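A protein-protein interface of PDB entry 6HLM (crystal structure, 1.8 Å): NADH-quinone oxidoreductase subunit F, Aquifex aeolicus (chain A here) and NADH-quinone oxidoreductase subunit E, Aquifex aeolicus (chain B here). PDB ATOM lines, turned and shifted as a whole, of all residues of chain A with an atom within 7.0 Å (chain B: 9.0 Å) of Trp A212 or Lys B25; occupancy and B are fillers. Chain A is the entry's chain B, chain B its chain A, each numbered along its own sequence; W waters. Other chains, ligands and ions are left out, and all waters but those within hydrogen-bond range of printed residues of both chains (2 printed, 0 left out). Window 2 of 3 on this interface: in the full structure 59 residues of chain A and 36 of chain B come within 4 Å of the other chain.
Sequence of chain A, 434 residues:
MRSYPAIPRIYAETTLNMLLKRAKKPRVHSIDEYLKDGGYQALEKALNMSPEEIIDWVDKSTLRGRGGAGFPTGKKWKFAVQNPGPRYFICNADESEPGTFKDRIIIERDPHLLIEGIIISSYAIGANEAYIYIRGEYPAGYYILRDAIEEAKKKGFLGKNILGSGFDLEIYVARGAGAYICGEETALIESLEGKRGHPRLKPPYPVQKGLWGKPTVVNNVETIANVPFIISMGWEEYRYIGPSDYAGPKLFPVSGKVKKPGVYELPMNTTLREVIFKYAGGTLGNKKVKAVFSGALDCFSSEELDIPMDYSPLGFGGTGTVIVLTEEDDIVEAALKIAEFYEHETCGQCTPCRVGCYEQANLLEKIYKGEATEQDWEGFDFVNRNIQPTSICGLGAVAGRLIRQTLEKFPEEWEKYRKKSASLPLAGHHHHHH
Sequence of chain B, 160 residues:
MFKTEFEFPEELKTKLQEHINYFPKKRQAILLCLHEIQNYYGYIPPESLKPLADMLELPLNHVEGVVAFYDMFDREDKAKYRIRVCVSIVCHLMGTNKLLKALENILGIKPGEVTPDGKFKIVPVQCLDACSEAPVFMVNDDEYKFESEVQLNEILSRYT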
ATOM      1  N   TYR A  88      23.747 -14.016 -10.645  1.00  0.00           N
ATOM      2  CA  TYR A  88      23.734 -14.875  -9.461  1.00  0.00           C
ATOM      3  C   TYR A  88      24.524 -14.258  -8.355  1.00  0.00           C
ATOM      4  O   TYR A  88      25.496 -13.542  -8.609  1.00  0.00           O
ATOM      5  CB  TYR A  88      24.302 -16.274  -9.806  1.00  0.00           C
ATOM      6  CG  TYR A  88      23.492 -17.010 -10.850  1.00  0.00           C
ATOM      7  CD1 TYR A  88      24.020 -17.276 -12.112  1.00  0.00           C
ATOM      8  CD2 TYR A  88      22.163 -17.362 -10.613  1.00  0.00           C
ATOM      9  CE1 TYR A  88      23.271 -17.942 -13.086  1.00  0.00           C
ATOM     10  CE2 TYR A  88      21.407 -18.038 -11.575  1.00  0.00           C
ATOM     11  CZ  TYR A  88      21.964 -18.313 -12.812  1.00  0.00           C
ATOM     12  OH  TYR A  88      21.210 -18.968 -13.755  1.00  0.00           O
ATOM     13  N   GLU A 129      18.382 -15.689  -7.714  1.00  0.00           N
ATOM     14  CA  GLU A 129      18.885 -16.957  -7.252  1.00  0.00           C
ATOM     15  C   GLU A 129      20.193 -16.681  -6.534  1.00  0.00           C
ATOM     16  O   GLU A 129      21.095 -16.053  -7.093  1.00  0.00           O
ATOM     17  CB  GLU A 129      19.064 -17.900  -8.444  1.00  0.00           C
ATOM     18  CG  GLU A 129      19.551 -19.314  -8.206  1.00  0.00           C
ATOM     19  CD  GLU A 129      19.425 -20.159  -9.468  1.00  0.00           C
ATOM     20  OE1 GLU A 129      18.403 -20.028 -10.174  1.00  0.00           O
ATOM     21  OE2 GLU A 129      20.354 -20.942  -9.762  1.00  0.00           O
ATOM     22  N   TYR A 131      23.212 -18.470  -3.634  1.00  0.00           N
ATOM     23  CA  TYR A 131      23.735 -19.714  -3.079  1.00  0.00           C
ATOM     24  C   TYR A 131      24.582 -19.452  -1.869  1.00  0.00           C
ATOM     25  O   TYR A 131      25.242 -18.423  -1.798  1.00  0.00           O
ATOM     26  CB  TYR A 131      24.632 -20.408  -4.131  1.00  0.00           C
ATOM     27  CG  TYR A 131      23.853 -20.970  -5.282  1.00  0.00           C
ATOM     28  CD1 TYR A 131      23.527 -20.183  -6.380  1.00  0.00           C
ATOM     29  CD2 TYR A 131      23.414 -22.291  -5.266  1.00  0.00           C
ATOM     30  CE1 TYR A 131      22.765 -20.694  -7.428  1.00  0.00           C
ATOM     31  CE2 TYR A 131      22.670 -22.815  -6.310  1.00  0.00           C
ATOM     32  CZ  TYR A 131      22.356 -22.019  -7.391  1.00  0.00           C
ATOM     33  OH  TYR A 131      21.684 -22.605  -8.413  1.00  0.00           O
ATOM     34  N   ILE A 189      32.433 -22.125  -7.946  1.00  0.00           N
ATOM     35  CA  ILE A 189      31.448 -22.118  -9.032  1.00  0.00           C
ATOM     36  C   ILE A 189      31.437 -23.488  -9.768  1.00  0.00           C
ATOM     37  O   ILE A 189      30.359 -24.051  -9.989  1.00  0.00           O
ATOM     38  CB  ILE A 189      31.671 -20.923  -9.991  1.00  0.00           C
ATOM     39  CG1 ILE A 189      31.243 -19.599  -9.276  1.00  0.00           C
ATOM     40  CG2 ILE A 189      30.858 -21.111 -11.307  1.00  0.00           C
ATOM     41  CD1 ILE A 189      31.858 -18.303  -9.853  1.00  0.00           C
ATOM     42  N   LEU A 192      29.574 -25.841  -7.649  1.00  0.00           N
ATOM     43  CA  LEU A 192      28.142 -25.534  -7.655  1.00  0.00           C
ATOM     44  C   LEU A 192      27.491 -26.059  -8.915  1.00  0.00           C
ATOM     45  O   LEU A 192      26.285 -26.289  -8.921  1.00  0.00           O
ATOM     46  CB  LEU A 192      27.907 -24.021  -7.595  1.00  0.00           C
ATOM     47  CG  LEU A 192      27.764 -23.359  -6.243  1.00  0.00           C
ATOM     48  CD1 LEU A 192      27.431 -21.898  -6.427  1.00  0.00           C
ATOM     49  CD2 LEU A 192      26.658 -24.003  -5.417  1.00  0.00           C
ATOM     50  N   GLU A 193      28.276 -26.192 -10.005  1.00  0.00           N
ATOM     51  CA  GLU A 193      27.802 -26.732 -11.279  1.00  0.00           C
ATOM     52  C   GLU A 193      27.797 -28.276 -11.290  1.00  0.00           C
ATOM     53  O   GLU A 193      27.408 -28.874 -12.295  1.00  0.00           O
ATOM     54  CB  GLU A 193      28.622 -26.167 -12.444  1.00  0.00           C
ATOM     55  CG  GLU A 193      28.392 -24.691 -12.696  1.00  0.00           C
ATOM     56  CD  GLU A 193      29.244 -24.042 -13.768  1.00  0.00           C
ATOM     57  OE1 GLU A 193      29.012 -22.847 -14.047  1.00  0.00           O
ATOM     58  OE2 GLU A 193      30.129 -24.719 -14.338  1.00  0.00           O
ATOM     59  N   GLY A 194      28.252 -28.891 -10.197  1.00  0.00           N
ATOM     60  CA  GLY A 194      28.275 -30.339 -10.039  1.00  0.00           C
ATOM     61  C   GLY A 194      29.530 -31.024 -10.553  1.00  0.00           C
ATOM     62  O   GLY A 194      29.511 -32.221 -10.851  1.00  0.00           O
ATOM     63  N   LYS A 195      30.630 -30.277 -10.632  1.00  0.00           N
ATOM     64  CA  LYS A 195      31.897 -30.782 -11.142  1.00  0.00           C
ATOM     65  C   LYS A 195      32.972 -30.799 -10.086  1.00  0.00           C
ATOM     66  O   LYS A 195      32.740 -30.369  -8.941  1.00  0.00           O
ATOM     67  CB  LYS A 195      32.351 -29.941 -12.356  1.00  0.00           C
ATOM     68  CG  LYS A 195      31.444 -30.112 -13.592  1.00  0.00           C
ATOM     69  CD  LYS A 195      31.803 -29.131 -14.708  1.00  0.00           C
ATOM     70  CE  LYS A 195      31.237 -27.754 -14.451  1.00  0.00           C
ATOM     71  NZ  LYS A 195      31.754 -26.731 -15.411  1.00  0.00           N
ATOM     72  N   ARG A 200      39.242 -21.766 -12.657  1.00  0.00           N
ATOM     73  CA  ARG A 200      39.246 -21.364 -14.072  1.00  0.00           C
ATOM     74  C   ARG A 200      40.271 -20.283 -14.269  1.00  0.00           C
ATOM     75  O   ARG A 200      40.577 -19.538 -13.341  1.00  0.00           O
ATOM     76  CB  ARG A 200      37.873 -20.765 -14.461  1.00  0.00           C
ATOM     77  CG  ARG A 200      36.672 -21.645 -14.202  1.00  0.00           C
ATOM     78  CD  ARG A 200      35.428 -20.829 -14.469  1.00  0.00           C
ATOM     79  NE  ARG A 200      34.218 -21.653 -14.427  1.00  0.00           N
ATOM     80  CZ  ARG A 200      32.980 -21.181 -14.500  1.00  0.00           C
ATOM     81  NH1 ARG A 200      32.764 -19.876 -14.603  1.00  0.00           N
ATOM     82  NH2 ARG A 200      31.947 -22.009 -14.457  1.00  0.00           N
ATOM     83  N   LYS A 209      31.584 -13.584 -16.208  1.00  0.00           N
ATOM     84  CA  LYS A 209      31.217 -14.952 -16.568  1.00  0.00           C
ATOM     85  C   LYS A 209      31.453 -15.817 -15.344  1.00  0.00           C
ATOM     86  O   LYS A 209      32.600 -16.020 -14.942  1.00  0.00           O
ATOM     87  CB  LYS A 209      32.096 -15.396 -17.770  1.00  0.00           C
ATOM     88  CG  LYS A 209      31.889 -16.823 -18.259  1.00  0.00           C
ATOM     89  CD  LYS A 209      32.516 -17.027 -19.646  1.00  0.00           C
ATOM     90  CE  LYS A 209      32.413 -18.452 -20.143  1.00  0.00           C
ATOM     91  NZ  LYS A 209      31.002 -18.882 -20.377  1.00  0.00           N
ATOM     92  N   GLY A 210      30.372 -16.280 -14.739  1.00  0.00           N
ATOM     93  CA  GLY A 210      30.437 -17.045 -13.495  1.00  0.00           C
ATOM     94  C   GLY A 210      29.660 -18.330 -13.555  1.00  0.00           C
ATOM     95  O   GLY A 210      29.937 -19.193 -14.400  1.00  0.00           O
ATOM     96  N   LEU A 211      28.657 -18.448 -12.666  1.00  0.00           N
ATOM     97  CA  LEU A 211      27.778 -19.610 -12.630  1.00  0.00           C
ATOM     98  C   LEU A 211      26.995 -19.704 -13.942  1.00  0.00           C
ATOM     99  O   LEU A 211      26.322 -18.749 -14.317  1.00  0.00           O
ATOM    100  CB  LEU A 211      26.814 -19.496 -11.439  1.00  0.00           C
ATOM    101  CG  LEU A 211      25.910 -20.719 -11.214  1.00  0.00           C
ATOM    102  CD1 LEU A 211      26.749 -21.970 -10.851  1.00  0.00           C
ATOM    103  CD2 LEU A 211      24.909 -20.455 -10.103  1.00  0.00           C
ATOM    104  N   TRP A 212      27.115 -20.854 -14.645  1.00  0.00           N
ATOM    105  CA  TRP A 212      26.494 -21.098 -15.960  1.00  0.00           C
ATOM    106  C   TRP A 212      26.888 -20.008 -16.962  1.00  0.00           C
ATOM    107  O   TRP A 212      26.108 -19.673 -17.864  1.00  0.00           O
ATOM    108  CB  TRP A 212      24.944 -21.238 -15.846  1.00  0.00           C
ATOM    109  CG  TRP A 212      24.472 -22.135 -14.741  1.00  0.00           C
ATOM    110  CD1 TRP A 212      23.641 -21.800 -13.706  1.00  0.00           C
ATOM    111  CD2 TRP A 212      24.820 -23.511 -14.546  1.00  0.00           C
ATOM    112  NE1 TRP A 212      23.453 -22.884 -12.878  1.00  0.00           N
ATOM    113  CE2 TRP A 212      24.152 -23.952 -13.381  1.00  0.00           C
ATOM    114  CE3 TRP A 212      25.590 -24.437 -15.283  1.00  0.00           C
ATOM    115  CZ2 TRP A 212      24.266 -25.258 -12.905  1.00  0.00           C
ATOM    116  CZ3 TRP A 212      25.696 -25.735 -14.815  1.00  0.00           C
ATOM    117  CH2 TRP A 212      25.036 -26.136 -13.640  1.00  0.00           C
ATOM    118  N   GLY A 213      28.069 -19.433 -16.747  1.00  0.00           N
ATOM    119  CA  GLY A 213      28.648 -18.375 -17.571  1.00  0.00           C
ATOM    120  C   GLY A 213      27.954 -17.033 -17.470  1.00  0.00           C
ATOM    121  O   GLY A 213      28.177 -16.157 -18.315  1.00  0.00           O
ATOM    122  N   LYS A 214      27.087 -16.867 -16.450  1.00  0.00           N
ATOM    123  CA  LYS A 214      26.336 -15.633 -16.235  1.00  0.00           C
ATOM    124  C   LYS A 214      27.048 -14.705 -15.243  1.00  0.00           C
ATOM    125  O   LYS A 214      27.804 -15.208 -14.420  1.00  0.00           O
ATOM    126  CB  LYS A 214      24.911 -15.963 -15.730  1.00  0.00           C
ATOM    127  CG  LYS A 214      24.014 -16.722 -16.742  1.00  0.00           C
ATOM    128  CD  LYS A 214      23.529 -15.824 -17.876  1.00  0.00           C
ATOM    129  CE  LYS A 214      22.919 -16.602 -19.014  1.00  0.00           C
ATOM    130  NZ  LYS A 214      22.549 -15.709 -20.146  1.00  0.00           N
ATOM    131  N   PRO A 215      26.764 -13.364 -15.264  1.00  0.00           N
ATOM    132  CA  PRO A 215      27.356 -12.455 -14.259  1.00  0.00           C
ATOM    133  C   PRO A 215      27.076 -12.965 -12.843  1.00  0.00           C
ATOM    134  O   PRO A 215      25.931 -13.249 -12.501  1.00  0.00           O
ATOM    135  CB  PRO A 215      26.628 -11.123 -14.523  1.00  0.00           C
ATOM    136  CG  PRO A 215      26.266 -11.197 -15.987  1.00  0.00           C
ATOM    137  CD  PRO A 215      25.872 -12.622 -16.191  1.00  0.00           C
ATOM    138  N   THR A 216      28.130 -13.141 -12.049  1.00  0.00           N
ATOM    139  CA  THR A 216      28.016 -13.714 -10.712  1.00  0.00           C
ATOM    140  C   THR A 216      28.865 -12.929  -9.723  1.00  0.00           C
ATOM    141  O   THR A 216      30.042 -12.699  -9.984  1.00  0.00           O
ATOM    142  CB  THR A 216      28.505 -15.196 -10.757  1.00  0.00           C
ATOM    143  OG1 THR A 216      27.724 -15.943 -11.697  1.00  0.00           O
ATOM    144  CG2 THR A 216      28.471 -15.877  -9.369  1.00  0.00           C
ATOM    145  N   HIS B  19      17.198 -34.165  -2.732  1.00  0.00           N
ATOM    146  CA  HIS B  19      18.384 -33.371  -3.076  1.00  0.00           C
ATOM    147  C   HIS B  19      18.380 -33.025  -4.568  1.00  0.00           C
ATOM    148  O   HIS B  19      18.654 -31.880  -4.930  1.00  0.00           O
ATOM    149  CB  HIS B  19      19.682 -34.114  -2.708  1.00  0.00           C
ATOM    150  CG  HIS B  19      19.912 -34.307  -1.238  1.00  0.00           C
ATOM    151  ND1 HIS B  19      19.788 -33.262  -0.338  1.00  0.00           N
ATOM    152  CD2 HIS B  19      20.289 -35.421  -0.562  1.00  0.00           C
ATOM    153  CE1 HIS B  19      20.076 -33.771   0.851  1.00  0.00           C
ATOM    154  NE2 HIS B  19      20.400 -35.063   0.764  1.00  0.00           N
ATOM    155  N   ILE B  20      18.050 -34.019  -5.428  1.00  0.00           N
ATOM    156  CA  ILE B  20      18.016 -33.889  -6.886  1.00  0.00           C
ATOM    157  C   ILE B  20      16.998 -32.805  -7.323  1.00  0.00           C
ATOM    158  O   ILE B  20      17.308 -31.988  -8.198  1.00  0.00           O
ATOM    159  CB  ILE B  20      17.804 -35.290  -7.540  1.00  0.00           C
ATOM    160  CG1 ILE B  20      19.137 -36.083  -7.489  1.00  0.00           C
ATOM    161  CG2 ILE B  20      17.301 -35.193  -8.997  1.00  0.00           C
ATOM    162  CD1 ILE B  20      19.017 -37.593  -7.588  1.00  0.00           C
ATOM    163  N   ASN B  21      15.839 -32.754  -6.660  1.00  0.00           N
ATOM    164  CA  ASN B  21      14.802 -31.761  -6.948  1.00  0.00           C
ATOM    165  C   ASN B  21      15.010 -30.414  -6.230  1.00  0.00           C
ATOM    166  O   ASN B  21      14.261 -29.468  -6.503  1.00  0.00           O
ATOM    167  CB  ASN B  21      13.426 -32.330  -6.602  1.00  0.00           C
ATOM    168  CG  ASN B  21      13.018 -33.474  -7.495  1.00  0.00           C
ATOM    169  OD1 ASN B  21      13.150 -33.420  -8.725  1.00  0.00           O
ATOM    170  ND2 ASN B  21      12.511 -34.533  -6.888  1.00  0.00           N
ATOM    171  N   TYR B  22      16.018 -30.324  -5.329  1.00  0.00           N
ATOM    172  CA  TYR B  22      16.287 -29.107  -4.551  1.00  0.00           C
ATOM    173  C   TYR B  22      16.857 -27.951  -5.390  1.00  0.00           C
ATOM    174  O   TYR B  22      16.313 -26.852  -5.330  1.00  0.00           O
ATOM    175  CB  TYR B  22      17.184 -29.420  -3.340  1.00  0.00           C
ATOM    176  CG  TYR B  22      17.624 -28.224  -2.515  1.00  0.00           C
ATOM    177  CD1 TYR B  22      16.740 -27.589  -1.639  1.00  0.00           C
ATOM    178  CD2 TYR B  22      18.958 -27.828  -2.489  1.00  0.00           C
ATOM    179  CE1 TYR B  22      17.151 -26.513  -0.847  1.00  0.00           C
ATOM    180  CE2 TYR B  22      19.381 -26.763  -1.702  1.00  0.00           C
ATOM    181  CZ  TYR B  22      18.480 -26.109  -0.879  1.00  0.00           C
ATOM    182  OH  TYR B  22      18.939 -25.097  -0.074  1.00  0.00           O
ATOM    183  N   PHE B  23      17.949 -28.171  -6.141  1.00  0.00           N
ATOM    184  CA  PHE B  23      18.562 -27.099  -6.934  1.00  0.00           C
ATOM    185  C   PHE B  23      17.856 -26.927  -8.268  1.00  0.00           C
ATOM    186  O   PHE B  23      17.218 -27.886  -8.713  1.00  0.00           O
ATOM    187  CB  PHE B  23      20.047 -27.409  -7.207  1.00  0.00           C
ATOM    188  CG  PHE B  23      20.908 -27.500  -5.971  1.00  0.00           C
ATOM    189  CD1 PHE B  23      21.349 -26.352  -5.326  1.00  0.00           C
ATOM    190  CD2 PHE B  23      21.288 -28.736  -5.457  1.00  0.00           C
ATOM    191  CE1 PHE B  23      22.149 -26.434  -4.183  1.00  0.00           C
ATOM    192  CE2 PHE B  23      22.080 -28.819  -4.308  1.00  0.00           C
ATOM    193  CZ  PHE B  23      22.487 -27.663  -3.667  1.00  0.00           C
ATOM    194  N   PRO B  24      18.027 -25.778  -8.985  1.00  0.00           N
ATOM    195  CA  PRO B  24      17.404 -25.642 -10.317  1.00  0.00           C
ATOM    196  C   PRO B  24      17.818 -26.742 -11.307  1.00  0.00           C
ATOM    197  O   PRO B  24      17.018 -27.113 -12.147  1.00  0.00           O
ATOM    198  CB  PRO B  24      17.892 -24.266 -10.780  1.00  0.00           C
ATOM    199  CG  PRO B  24      18.098 -23.502  -9.495  1.00  0.00           C
ATOM    200  CD  PRO B  24      18.698 -24.518  -8.586  1.00  0.00           C
ATOM    201  N   LYS B  25      19.067 -27.266 -11.204  1.00  0.00           N
ATOM    202  CA  LYS B  25      19.574 -28.326 -12.084  1.00  0.00           C
ATOM    203  C   LYS B  25      19.963 -29.553 -11.262  1.00  0.00           C
ATOM    204  O   LYS B  25      20.597 -29.413 -10.223  1.00  0.00           O
ATOM    205  CB  LYS B  25      20.740 -27.832 -12.964  1.00  0.00           C
ATOM    206  CG  LYS B  25      20.352 -26.679 -13.897  1.00  0.00           C
ATOM    207  CD  LYS B  25      21.456 -26.362 -14.912  1.00  0.00           C
ATOM    208  CE  LYS B  25      21.344 -24.947 -15.436  1.00  0.00           C
ATOM    209  NZ  LYS B  25      22.301 -24.680 -16.551  1.00  0.00           N
ATOM    210  N   LYS B  26      19.574 -30.747 -11.730  1.00  0.00           N
ATOM    211  CA  LYS B  26      19.812 -32.042 -11.072  1.00  0.00           C
ATOM    212  C   LYS B  26      21.272 -32.290 -10.700  1.00  0.00           C
ATOM    213  O   LYS B  26      21.546 -32.727  -9.585  1.00  0.00           O
ATOM    214  CB  LYS B  26      19.311 -33.210 -11.950  1.00  0.00           C
ATOM    215  CG  LYS B  26      17.800 -33.209 -12.157  1.00  0.00           C
ATOM    216  CD  LYS B  26      17.303 -34.488 -12.807  1.00  0.00           C
ATOM    217  CE  LYS B  26      15.793 -34.544 -12.767  1.00  0.00           C
ATOM    218  NZ  LYS B  26      15.286 -35.896 -13.098  1.00  0.00           N
ATOM    219  N   ARG B  27      22.200 -32.031 -11.634  1.00  0.00           N
ATOM    220  CA  ARG B  27      23.635 -32.288 -11.439  1.00  0.00           C
ATOM    221  C   ARG B  27      24.255 -31.507 -10.270  1.00  0.00           C
ATOM    222  O   ARG B  27      25.290 -31.923  -9.739  1.00  0.00           O
ATOM    223  CB  ARG B  27      24.431 -32.083 -12.739  1.00  0.00           C
ATOM    224  CG  ARG B  27      24.421 -30.669 -13.328  1.00  0.00           C
ATOM    225  CD  ARG B  27      25.009 -30.781 -14.727  1.00  0.00           C
ATOM    226  NE  ARG B  27      25.011 -29.548 -15.519  1.00  0.00           N
ATOM    227  CZ  ARG B  27      23.983 -29.097 -16.238  1.00  0.00           C
ATOM    228  NH1 ARG B  27      22.814 -29.721 -16.204  1.00  0.00           N
ATOM    229  NH2 ARG B  27      24.109 -27.996 -16.970  1.00  0.00           N
ATOM    230  N   GLN B  28      23.619 -30.404  -9.842  1.00  0.00           N
ATOM    231  CA  GLN B  28      24.107 -29.591  -8.724  1.00  0.00           C
ATOM    232  C   GLN B  28      24.028 -30.339  -7.399  1.00  0.00           C
ATOM    233  O   GLN B  28      24.749 -30.007  -6.466  1.00  0.00           O
ATOM    234  CB  GLN B  28      23.356 -28.260  -8.631  1.00  0.00           C
ATOM    235  CG  GLN B  28      23.492 -27.377  -9.872  1.00  0.00           C
ATOM    236  CD  GLN B  28      22.850 -26.034  -9.641  1.00  0.00           C
ATOM    237  OE1 GLN B  28      21.691 -25.813  -9.995  1.00  0.00           O
ATOM    238  NE2 GLN B  28      23.590 -25.101  -9.092  1.00  0.00           N
ATOM    239  N   ALA B  29      23.174 -31.379  -7.332  1.00  0.00           N
ATOM    240  CA  ALA B  29      22.958 -32.191  -6.129  1.00  0.00           C
ATOM    241  C   ALA B  29      23.995 -33.310  -5.893  1.00  0.00           C
ATOM    242  O   ALA B  29      23.868 -34.030  -4.913  1.00  0.00           O
ATOM    243  CB  ALA B  29      21.563 -32.803  -6.191  1.00  0.00           C
ATOM    244  N   ILE B  30      25.007 -33.456  -6.773  1.00  0.00           N
ATOM    245  CA  ILE B  30      25.991 -34.552  -6.697  1.00  0.00           C
ATOM    246  C   ILE B  30      26.640 -34.706  -5.302  1.00  0.00           C
ATOM    247  O   ILE B  30      26.700 -35.826  -4.792  1.00  0.00           O
ATOM    248  CB  ILE B  30      27.061 -34.498  -7.830  1.00  0.00           C
ATOM    249  CG1 ILE B  30      27.917 -35.808  -7.851  1.00  0.00           C
ATOM    250  CG2 ILE B  30      27.946 -33.220  -7.773  1.00  0.00           C
ATOM    251  CD1 ILE B  30      28.562 -36.170  -9.199  1.00  0.00           C
ATOM    252  N   MET B  55      20.279 -41.104 -11.966  1.00  0.00           N
ATOM    253  CA  MET B  55      19.432 -40.159 -11.225  1.00  0.00           C
ATOM    254  C   MET B  55      19.846 -38.697 -11.439  1.00  0.00           C
ATOM    255  O   MET B  55      18.982 -37.822 -11.482  1.00  0.00           O
ATOM    256  CB  MET B  55      19.451 -40.488  -9.729  1.00  0.00           C
ATOM    257  CG  MET B  55      18.647 -41.706  -9.344  1.00  0.00           C
ATOM    258  SD  MET B  55      18.917 -42.095  -7.596  1.00  0.00           S
ATOM    259  CE  MET B  55      17.548 -41.221  -6.863  1.00  0.00           C
ATOM    260  N   LEU B  56      21.161 -38.434 -11.554  1.00  0.00           N
ATOM    261  CA  LEU B  56      21.725 -37.090 -11.769  1.00  0.00           C
ATOM    262  C   LEU B  56      21.775 -36.728 -13.265  1.00  0.00           C
ATOM    263  O   LEU B  56      22.047 -35.573 -13.611  1.00  0.00           O
ATOM    264  CB  LEU B  56      23.150 -37.022 -11.185  1.00  0.00           C
ATOM    265  CG  LEU B  56      23.288 -37.103  -9.650  1.00  0.00           C
ATOM    266  CD1 LEU B  56      24.721 -37.351  -9.252  1.00  0.00           C
ATOM    267  CD2 LEU B  56      22.782 -35.841  -8.970  1.00  0.00           C
ATOM    268  N   GLU B  57      21.536 -37.724 -14.140  1.00  0.00           N
ATOM    269  CA  GLU B  57      21.577 -37.650 -15.619  1.00  0.00           C
ATOM    270  C   GLU B  57      22.989 -37.263 -16.083  1.00  0.00           C
ATOM    271  O   GLU B  57      23.174 -36.413 -16.958  1.00  0.00           O
ATOM    272  CB  GLU B  57      20.469 -36.736 -16.194  1.00  0.00           C
ATOM    273  CG  GLU B  57      19.052 -37.217 -15.902  1.00  0.00           C
ATOM    274  CD  GLU B  57      17.921 -36.237 -16.171  1.00  0.00           C
ATOM    275  OE1 GLU B  57      18.185 -35.136 -16.707  1.00  0.00           O
ATOM    276  OE2 GLU B  57      16.760 -36.581 -15.855  1.00  0.00           O
ATOM    277  N   LEU B  58      23.992 -37.898 -15.463  1.00  0.00           N
ATOM    278  CA  LEU B  58      25.409 -37.667 -15.736  1.00  0.00           C
ATOM    279  C   LEU B  58      26.103 -38.954 -16.189  1.00  0.00           C
ATOM    280  O   LEU B  58      25.663 -40.036 -15.805  1.00  0.00           O
ATOM    281  CB  LEU B  58      26.110 -37.149 -14.463  1.00  0.00           C
ATOM    282  CG  LEU B  58      25.770 -35.727 -13.990  1.00  0.00           C
ATOM    283  CD1 LEU B  58      26.384 -35.452 -12.617  1.00  0.00           C
ATOM    284  CD2 LEU B  58      26.220 -34.664 -15.008  1.00  0.00           C
ATOM    285  N   HIS B  62      31.899 -39.152 -14.940  1.00  0.00           N
ATOM    286  CA  HIS B  62      31.801 -37.843 -14.259  1.00  0.00           C
ATOM    287  C   HIS B  62      31.657 -38.070 -12.739  1.00  0.00           C
ATOM    288  O   HIS B  62      32.378 -37.449 -11.949  1.00  0.00           O
ATOM    289  CB  HIS B  62      30.606 -37.047 -14.834  1.00  0.00           C
ATOM    290  CG  HIS B  62      30.383 -35.678 -14.261  1.00  0.00           C
ATOM    291  ND1 HIS B  62      30.072 -34.606 -15.075  1.00  0.00           N
ATOM    292  CD2 HIS B  62      30.382 -35.257 -12.970  1.00  0.00           C
ATOM    293  CE1 HIS B  62      29.911 -33.578 -14.261  1.00  0.00           C
ATOM    294  NE2 HIS B  62      30.104 -33.922 -12.988  1.00  0.00           N
HETATM  295  O   HOH W   1      21.252 -23.329 -11.048  1.00  0.00           O
HETATM  296  O   HOH W   2      27.751 -28.747 -15.079  1.00  0.00           O
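NE2 of Gln B28 sits at hydrogen-bond distance from O of Leu A192 (3.0 Å).
NE2 of Gln B28 is in hydrogen-bond range of OH of Tyr A131, at 3.2 Å.
The backbone carbonyl oxygen (O) of Gly A194 is in hydrogen-bond range of a ring nitrogen (NE2) of His B62, 2.8 Å away.
The side-chain carboxylate (OE1) of Glu A193 is in salt-bridge range of the guanidinium group (NH2) of Arg A200.
The side-chain amide oxygen of Gln B28 sits at hydrogen-bond distance from the backbone NH of Lys B25 (3.2 Å).
The side-chain amino group (NZ) of Lys A195 lies within salt-bridge range of the side-chain carboxylate (OE2) of Glu A193, 2.8 Å away.
The backbone NH (N) of Trp A212 lies within hydrogen-bond range of the side-chain carboxylate (OE1) of Glu A193 (2.8 Å).
The side-chain hydroxyl (OH) of Tyr A131 lies within hydrogen-bond range of the side-chain carboxylate (OE2) of Glu A129, 2.5 Å away.
Among the printed residues, pairs that only touch across the chains: Glu A129 with Pro B24 (3.4 Å), Tyr A131 with Phe B23 (3.9 Å), Tyr A131 with Pro B24 (3.6 Å), Glu A193 with Arg B27 (3.6 Å), Gly A194 with Arg B27 (3.4 Å), Gly A194 with Ile B30 (3.6 Å), Lys A195 with His B62 (3.8 Å), Trp A212 with Lys B25 (3.4 Å), Trp A212 with Arg B27 (3.5 Å) and Trp A212 with Gln B28 (3.6 Å).
Of the printed residues of chain B, Glu A129 touches Pro B24 (3.4 Å).
Glu A193 touches just one residue of chain B: Arg B27.
Lys A209 touches none of the printed residues of chain B.
Of chain B, only Lys B25 (3.4 Å), Arg B27 (3.5 Å) and Gln B28 (3.6 Å) come within 4 Å of Trp A212.
Gly A213 touches none of the printed residues of chain B.
Of the printed residues of chain A, Phe B23 touches Tyr A131 (3.9 Å).
Of chain A, only Trp A212 comes within 4 Å of Lys B25.
Of the printed residues of chain A, Ile B30 touches Gly A194.
Met B55 touches none of the printed residues of chain A.
The nearest residue of chain A that does not touch Lys B25 is Tyr A131 (6.0 Å).
The nearest printed residue of chain B that does not touch Gly A194 is Gln B28 (4.4 Å).
Hydrophobic or aromatic side chains of chain A that line the printed part of chain B: Tyr A131 and Trp A212.
Among the printed residues, 13 pairs touch across the chains.
Among the printed residues, no Asp or Glu carboxylate lies within 4 Å of a Lys or Arg side-chain nitrogen of the other chain.
Water W1 lies within hydrogen-bond range of the side-chain amide oxygen (OE1) of Gln B28, the side-chain hydroxyl (OH) of Tyr A131, the side-chain carboxylate (OE2) of Glu A129 and the indole nitrogen (NE1) of Trp A212.
Water W2 bridges the backbone carbonyl oxygen of Glu A193 and the guanidinium group of Arg B27.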
